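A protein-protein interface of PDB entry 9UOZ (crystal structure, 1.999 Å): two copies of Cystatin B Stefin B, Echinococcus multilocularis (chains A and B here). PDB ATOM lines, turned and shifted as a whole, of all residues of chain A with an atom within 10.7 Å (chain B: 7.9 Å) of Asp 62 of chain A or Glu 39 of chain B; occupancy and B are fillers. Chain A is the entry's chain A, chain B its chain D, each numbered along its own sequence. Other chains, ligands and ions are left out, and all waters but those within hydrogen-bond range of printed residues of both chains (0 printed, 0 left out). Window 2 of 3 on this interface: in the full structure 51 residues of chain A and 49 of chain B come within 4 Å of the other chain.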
ATOM      1  N   LYS A  58      -5.773 -10.726   8.010  1.00  0.00           N
ATOM      2  CA  LYS A  58      -7.082 -10.755   7.373  1.00  0.00           C
ATOM      3  C   LYS A  58      -7.594 -12.193   7.383  1.00  0.00           C
ATOM      4  O   LYS A  58      -6.905 -13.100   6.886  1.00  0.00           O
ATOM      5  CB  LYS A  58      -6.928 -10.211   5.951  1.00  0.00           C
ATOM      6  CG  LYS A  58      -8.253  -9.983   5.238  1.00  0.00           C
ATOM      7  CD  LYS A  58      -8.160  -9.437   3.822  1.00  0.00           C
ATOM      8  CE  LYS A  58      -8.651  -8.026   3.612  1.00  0.00           C
ATOM      9  NZ  LYS A  58      -7.616  -7.020   3.804  1.00  0.00           N
ATOM     10  N   VAL A  59      -8.776 -12.391   7.957  1.00  0.00           N
ATOM     11  CA  VAL A  59      -9.285 -13.734   8.191  1.00  0.00           C
ATOM     12  C   VAL A  59     -10.711 -13.816   7.658  1.00  0.00           C
ATOM     13  O   VAL A  59     -11.557 -13.006   8.029  1.00  0.00           O
ATOM     14  CB  VAL A  59      -9.242 -14.221   9.659  1.00  0.00           C
ATOM     15  CG1 VAL A  59      -8.186 -13.522  10.523  1.00  0.00           C
ATOM     16  CG2 VAL A  59     -10.572 -14.326  10.361  1.00  0.00           C
ATOM     17  N   GLU A  60     -10.939 -14.769   6.749  1.00  0.00           N
ATOM     18  CA  GLU A  60     -12.229 -14.991   6.139  1.00  0.00           C
ATOM     19  C   GLU A  60     -12.817 -16.265   6.724  1.00  0.00           C
ATOM     20  O   GLU A  60     -12.148 -17.292   6.788  1.00  0.00           O
ATOM     21  CB  GLU A  60     -12.051 -15.008   4.618  1.00  0.00           C
ATOM     22  CG  GLU A  60     -11.914 -13.570   4.100  1.00  0.00           C
ATOM     23  CD  GLU A  60     -11.127 -13.260   2.835  1.00  0.00           C
ATOM     24  OE1 GLU A  60     -11.420 -13.924   1.806  1.00  0.00           O
ATOM     25  OE2 GLU A  60     -10.220 -12.374   2.913  1.00  0.00           O
ATOM     26  N   HIS A  61     -14.059 -16.155   7.196  1.00  0.00           N
ATOM     27  CA  HIS A  61     -14.739 -17.276   7.832  1.00  0.00           C
ATOM     28  C   HIS A  61     -16.215 -17.164   7.485  1.00  0.00           C
ATOM     29  O   HIS A  61     -16.821 -16.129   7.762  1.00  0.00           O
ATOM     30  CB  HIS A  61     -14.506 -17.336   9.353  1.00  0.00           C
ATOM     31  CG  HIS A  61     -14.918 -16.100  10.069  1.00  0.00           C
ATOM     32  ND1 HIS A  61     -15.832 -15.922  11.084  1.00  0.00           N
ATOM     33  CD2 HIS A  61     -14.394 -14.898   9.828  1.00  0.00           C
ATOM     34  CE1 HIS A  61     -15.879 -14.644  11.410  1.00  0.00           C
ATOM     35  NE2 HIS A  61     -14.992 -14.002  10.676  1.00  0.00           N
ATOM     36  N   ASP A  62     -16.731 -18.194   6.804  1.00  0.00           N
ATOM     37  CA  ASP A  62     -18.151 -18.339   6.499  1.00  0.00           C
ATOM     38  C   ASP A  62     -18.714 -17.063   5.872  1.00  0.00           C
ATOM     39  O   ASP A  62     -19.789 -16.622   6.236  1.00  0.00           O
ATOM     40  CB  ASP A  62     -18.920 -18.731   7.750  1.00  0.00           C
ATOM     41  CG  ASP A  62     -18.437 -19.997   8.439  1.00  0.00           C
ATOM     42  OD1 ASP A  62     -17.820 -20.845   7.753  1.00  0.00           O
ATOM     43  OD2 ASP A  62     -18.656 -20.105   9.662  1.00  0.00           O
ATOM     44  N   GLY A  63     -17.968 -16.464   4.937  1.00  0.00           N
ATOM     45  CA  GLY A  63     -18.428 -15.314   4.180  1.00  0.00           C
ATOM     46  C   GLY A  63     -18.330 -13.996   4.951  1.00  0.00           C
ATOM     47  O   GLY A  63     -18.878 -12.990   4.510  1.00  0.00           O
ATOM     48  N   ASN A  64     -17.617 -13.987   6.086  1.00  0.00           N
ATOM     49  CA  ASN A  64     -17.312 -12.752   6.796  1.00  0.00           C
ATOM     50  C   ASN A  64     -15.800 -12.540   6.798  1.00  0.00           C
ATOM     51  O   ASN A  64     -15.031 -13.465   6.610  1.00  0.00           O
ATOM     52  CB  ASN A  64     -17.924 -12.741   8.190  1.00  0.00           C
ATOM     53  CG  ASN A  64     -19.422 -12.857   8.115  1.00  0.00           C
ATOM     54  OD1 ASN A  64     -20.106 -11.903   7.734  1.00  0.00           O
ATOM     55  ND2 ASN A  64     -19.938 -14.018   8.467  1.00  0.00           N
ATOM     56  N   CYS A  65     -15.403 -11.292   6.995  1.00  0.00           N
ATOM     57  CA  CYS A  65     -14.000 -10.919   6.985  1.00  0.00           C
ATOM     58  C   CYS A  65     -13.721 -10.087   8.234  1.00  0.00           C
ATOM     59  O   CYS A  65     -14.373  -9.066   8.463  1.00  0.00           O
ATOM     60  CB  CYS A  65     -13.660 -10.161   5.706  1.00  0.00           C
ATOM     61  SG  CYS A  65     -11.930  -9.605   5.662  1.00  0.00           S
ATOM     62  N   TRP A  66     -12.769 -10.562   9.050  1.00  0.00           N
ATOM     63  CA  TRP A  66     -12.296  -9.827  10.216  1.00  0.00           C
ATOM     64  C   TRP A  66     -10.807  -9.521  10.050  1.00  0.00           C
ATOM     65  O   TRP A  66     -10.070 -10.311   9.440  1.00  0.00           O
ATOM     66  CB  TRP A  66     -12.469 -10.682  11.478  1.00  0.00           C
ATOM     67  CG  TRP A  66     -13.871 -10.863  11.978  1.00  0.00           C
ATOM     68  CD1 TRP A  66     -15.046 -10.501  11.381  1.00  0.00           C
ATOM     69  CD2 TRP A  66     -14.239 -11.556  13.190  1.00  0.00           C
ATOM     70  NE1 TRP A  66     -16.109 -10.893  12.148  1.00  0.00           N
ATOM     71  CE2 TRP A  66     -15.648 -11.547  13.259  1.00  0.00           C
ATOM     72  CE3 TRP A  66     -13.521 -12.184  14.210  1.00  0.00           C
ATOM     73  CZ2 TRP A  66     -16.344 -12.117  14.323  1.00  0.00           C
ATOM     74  CZ3 TRP A  66     -14.202 -12.743  15.268  1.00  0.00           C
ATOM     75  CH2 TRP A  66     -15.596 -12.723  15.313  1.00  0.00           C
ATOM     76  N   VAL A  91     -13.161  -7.497   2.432  1.00  0.00           N
ATOM     77  CA  VAL A  91     -12.047  -8.109   1.719  1.00  0.00           C
ATOM     78  C   VAL A  91     -11.175  -7.025   1.085  1.00  0.00           C
ATOM     79  O   VAL A  91      -9.954  -7.175   0.995  1.00  0.00           O
ATOM     80  CB  VAL A  91     -12.324  -9.221   0.691  1.00  0.00           C
ATOM     81  CG1 VAL A  91     -13.707  -9.831   0.795  1.00  0.00           C
ATOM     82  CG2 VAL A  91     -11.979  -8.867  -0.759  1.00  0.00           C
ATOM     83  N   LYS B  26      -9.030 -19.516  15.153  1.00  0.00           N
ATOM     84  CA  LYS B  26     -10.222 -20.353  15.092  1.00  0.00           C
ATOM     85  C   LYS B  26     -10.904 -20.427  16.461  1.00  0.00           C
ATOM     86  O   LYS B  26     -12.118 -20.208  16.567  1.00  0.00           O
ATOM     87  CB  LYS B  26      -9.801 -21.725  14.553  1.00  0.00           C
ATOM     88  CG  LYS B  26     -10.799 -22.538  13.743  1.00  0.00           C
ATOM     89  CD  LYS B  26     -10.073 -23.645  12.969  1.00  0.00           C
ATOM     90  CE  LYS B  26     -10.528 -23.991  11.574  1.00  0.00           C
ATOM     91  NZ  LYS B  26      -9.367 -24.534  10.867  1.00  0.00           N
ATOM     92  N   ILE B  29     -12.527 -17.010  17.317  1.00  0.00           N
ATOM     93  CA  ILE B  29     -13.774 -16.775  16.612  1.00  0.00           C
ATOM     94  C   ILE B  29     -14.884 -17.581  17.296  1.00  0.00           C
ATOM     95  O   ILE B  29     -15.954 -17.065  17.571  1.00  0.00           O
ATOM     96  CB  ILE B  29     -13.636 -17.088  15.107  1.00  0.00           C
ATOM     97  CG1 ILE B  29     -12.645 -16.162  14.409  1.00  0.00           C
ATOM     98  CG2 ILE B  29     -15.007 -16.975  14.435  1.00  0.00           C
ATOM     99  CD1 ILE B  29     -12.277 -16.609  13.006  1.00  0.00           C
ATOM    100  N   LEU B  33     -18.282 -15.924  18.794  1.00  0.00           N
ATOM    101  CA  LEU B  33     -19.572 -16.136  18.149  1.00  0.00           C
ATOM    102  C   LEU B  33     -20.413 -17.163  18.904  1.00  0.00           C
ATOM    103  O   LEU B  33     -21.607 -17.243  18.665  1.00  0.00           O
ATOM    104  CB  LEU B  33     -19.353 -16.574  16.705  1.00  0.00           C
ATOM    105  CG  LEU B  33     -18.691 -15.541  15.780  1.00  0.00           C
ATOM    106  CD1 LEU B  33     -18.720 -16.064  14.343  1.00  0.00           C
ATOM    107  CD2 LEU B  33     -19.363 -14.169  15.844  1.00  0.00           C
ATOM    108  N   ARG B  35     -19.985 -20.379  18.623  1.00  0.00           N
ATOM    109  CA  ARG B  35     -20.046 -21.596  17.833  1.00  0.00           C
ATOM    110  C   ARG B  35     -18.839 -21.656  16.904  1.00  0.00           C
ATOM    111  O   ARG B  35     -18.412 -20.636  16.357  1.00  0.00           O
ATOM    112  CB  ARG B  35     -21.329 -21.719  16.998  1.00  0.00           C
ATOM    113  CG  ARG B  35     -21.753 -20.465  16.254  1.00  0.00           C
ATOM    114  CD  ARG B  35     -22.154 -20.697  14.789  1.00  0.00           C
ATOM    115  NE  ARG B  35     -21.870 -19.516  13.964  1.00  0.00           N
ATOM    116  CZ  ARG B  35     -21.764 -19.500  12.632  1.00  0.00           C
ATOM    117  NH1 ARG B  35     -21.877 -20.624  11.947  1.00  0.00           N
ATOM    118  NH2 ARG B  35     -21.519 -18.363  12.009  1.00  0.00           N
ATOM    119  N   GLU B  36     -18.350 -22.878  16.685  1.00  0.00           N
ATOM    120  CA  GLU B  36     -17.177 -23.117  15.866  1.00  0.00           C
ATOM    121  C   GLU B  36     -17.473 -22.718  14.419  1.00  0.00           C
ATOM    122  O   GLU B  36     -18.494 -23.113  13.859  1.00  0.00           O
ATOM    123  CB  GLU B  36     -16.785 -24.595  15.934  1.00  0.00           C
ATOM    124  CG  GLU B  36     -16.062 -24.991  17.213  1.00  0.00           C
ATOM    125  CD  GLU B  36     -14.633 -25.314  16.839  1.00  0.00           C
ATOM    126  OE1 GLU B  36     -13.839 -24.401  16.561  1.00  0.00           O
ATOM    127  OE2 GLU B  36     -14.342 -26.521  16.746  1.00  0.00           O
ATOM    128  N   PRO B  37     -16.599 -21.908  13.780  1.00  0.00           N
ATOM    129  CA  PRO B  37     -16.771 -21.574  12.373  1.00  0.00           C
ATOM    130  C   PRO B  37     -16.448 -22.756  11.466  1.00  0.00           C
ATOM    131  O   PRO B  37     -15.680 -23.630  11.856  1.00  0.00           O
ATOM    132  CB  PRO B  37     -15.799 -20.417  12.173  1.00  0.00           C
ATOM    133  CG  PRO B  37     -14.694 -20.738  13.178  1.00  0.00           C
ATOM    134  CD  PRO B  37     -15.406 -21.283  14.380  1.00  0.00           C
ATOM    135  N   SER B  38     -17.022 -22.751  10.259  1.00  0.00           N
ATOM    136  CA  SER B  38     -16.885 -23.852   9.320  1.00  0.00           C
ATOM    137  C   SER B  38     -15.632 -23.681   8.469  1.00  0.00           C
ATOM    138  O   SER B  38     -14.792 -24.576   8.410  1.00  0.00           O
ATOM    139  CB  SER B  38     -18.106 -23.969   8.450  1.00  0.00           C
ATOM    140  OG  SER B  38     -19.296 -23.855   9.216  1.00  0.00           O
ATOM    141  N   GLU B  39     -15.516 -22.521   7.806  1.00  0.00           N
ATOM    142  CA  GLU B  39     -14.330 -22.203   7.025  1.00  0.00           C
ATOM    143  C   GLU B  39     -13.605 -21.034   7.685  1.00  0.00           C
ATOM    144  O   GLU B  39     -14.230 -20.011   7.945  1.00  0.00           O
ATOM    145  CB  GLU B  39     -14.682 -21.863   5.579  1.00  0.00           C
ATOM    146  CG  GLU B  39     -13.444 -21.573   4.738  1.00  0.00           C
ATOM    147  CD  GLU B  39     -13.623 -21.870   3.261  1.00  0.00           C
ATOM    148  OE1 GLU B  39     -14.745 -22.190   2.790  1.00  0.00           O
ATOM    149  OE2 GLU B  39     -12.591 -21.778   2.552  1.00  0.00           O
ATOM    150  N   VAL B  40     -12.310 -21.217   7.968  1.00  0.00           N
ATOM    151  CA  VAL B  40     -11.452 -20.146   8.437  1.00  0.00           C
ATOM    152  C   VAL B  40     -10.189 -20.174   7.593  1.00  0.00           C
ATOM    153  O   VAL B  40      -9.474 -21.163   7.580  1.00  0.00           O
ATOM    154  CB  VAL B  40     -11.086 -20.241   9.926  1.00  0.00           C
ATOM    155  CG1 VAL B  40     -10.155 -19.113  10.343  1.00  0.00           C
ATOM    156  CG2 VAL B  40     -12.322 -20.255  10.808  1.00  0.00           C
ATOM    157  N   LYS B  41      -9.914 -19.063   6.903  1.00  0.00           N
ATOM    158  CA  LYS B  41      -8.731 -18.925   6.079  1.00  0.00           C
ATOM    159  C   LYS B  41      -8.059 -17.588   6.392  1.00  0.00           C
ATOM    160  O   LYS B  41      -8.697 -16.536   6.324  1.00  0.00           O
ATOM    161  CB  LYS B  41      -9.180 -19.015   4.614  1.00  0.00           C
ATOM    162  CG  LYS B  41      -8.052 -19.017   3.605  1.00  0.00           C
ATOM    163  CD  LYS B  41      -8.417 -19.533   2.217  1.00  0.00           C
ATOM    164  CE  LYS B  41      -7.192 -19.827   1.397  1.00  0.00           C
ATOM    165  NZ  LYS B  41      -7.460 -20.791   0.322  1.00  0.00           N
ATOM    166  N   ILE B  42      -6.761 -17.620   6.701  1.00  0.00           N
ATOM    167  CA  ILE B  42      -5.975 -16.400   6.791  1.00  0.00           C
ATOM    168  C   ILE B  42      -5.530 -16.045   5.381  1.00  0.00           C
ATOM    169  O   ILE B  42      -4.806 -16.827   4.805  1.00  0.00           O
ATOM    170  CB  ILE B  42      -4.793 -16.581   7.758  1.00  0.00           C
ATOM    171  CG1 ILE B  42      -5.283 -17.035   9.134  1.00  0.00           C
ATOM    172  CG2 ILE B  42      -3.951 -15.292   7.848  1.00  0.00           C
ATOM    173  CD1 ILE B  42      -4.172 -17.347  10.104  1.00  0.00           C
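O of Trp 66 of chain A lies within hydrogen-bond range of N of Val 59 of chain A (2.9 Å).
O of Asp 62 of chain A lies within hydrogen-bond range of ND2 of Asn 64 of chain A (3.4 Å).
Of the printed residues of chain B, Asp 62 of chain A touches Arg 35, Pro 37, Ser 38 and Glu 39.
Of the printed residues of chain A, Glu 39 of chain B touches Glu 60, His 61 and Asp 62.
Of chain A, only Asp 62 (3.6 Å) comes within 4 Å of Pro 37 of chain B.
Of chain A, only Asp 62 (3.2 Å) comes within 4 Å of Ser 38 of chain B.
Val 40 of chain B touches just these residues of chain A: Glu 60 and His 61.
Of the printed residues of chain B, Lys 58 of chain A touches Lys 41 (3.9 Å) and Ile 42 (3.4 Å).
Printed residues of chain A within 4 Å of Lys 41 of chain B: Lys 58, Val 59 and Glu 60.
The nearest printed residue of chain B that does not touch Asp 62 of chain A is Glu 36 of chain B (5.2 Å).
N of Lys 41 of chain B is in hydrogen-bond range of O of Glu 60 of chain A (2.9 Å).
The guanidinium group (NH1) of Arg 35 of chain B is in salt-bridge range of the side-chain carboxylate (OD2) of Asp 62 of chain A (3.98 Å).
OD2 of Asp 62 of chain A is in hydrogen-bond range of N of Ser 38 of chain B (3.2 Å).
N of Glu 39 of chain B sits at hydrogen-bond distance from OD1 of Asp 62 of chain A, 2.8 Å away.
Hydrophobic or aromatic side chains of chain A within 4 Å of the printed part of chain B: Val 59, His 61 and Trp 66.
Along chain A the printed residues that touch a printed residue of chain B span positions 58 to 66.
Hydrophobic or aromatic side chains of chain B that line the printed part of chain A: Ile 29, Leu 33, Pro 37, Val 40 and Ile 42.
Among the printed residues, merely in contact across the chains: His 61 of chain A with Glu 39 of chain B, Glu 60 of chain A with Val 40 of chain B, Val 59 of chain A with Lys 41 of chain B, Lys 58 of chain A with Ile 42 of chain B, His 61 of chain A with Ile 29 of chain B, Asp 62 of chain A with Pro 37 of chain B, Glu 60 of chain A with Glu 39 of chain B, Trp 66 of chain A with Ile 29 of chain B, Val 59 of chain A with Ile 29 of chain B, Lys 58 of chain A with Lys 41 of chain B, His 61 of chain A with Val 40 of chain B and Trp 66 of chain A with Leu 33 of chain B.
No position is printed for both chains.
Of the 16 pairs that touch across the chains among the printed residues, none has its exchanged pair printed and touching as well.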
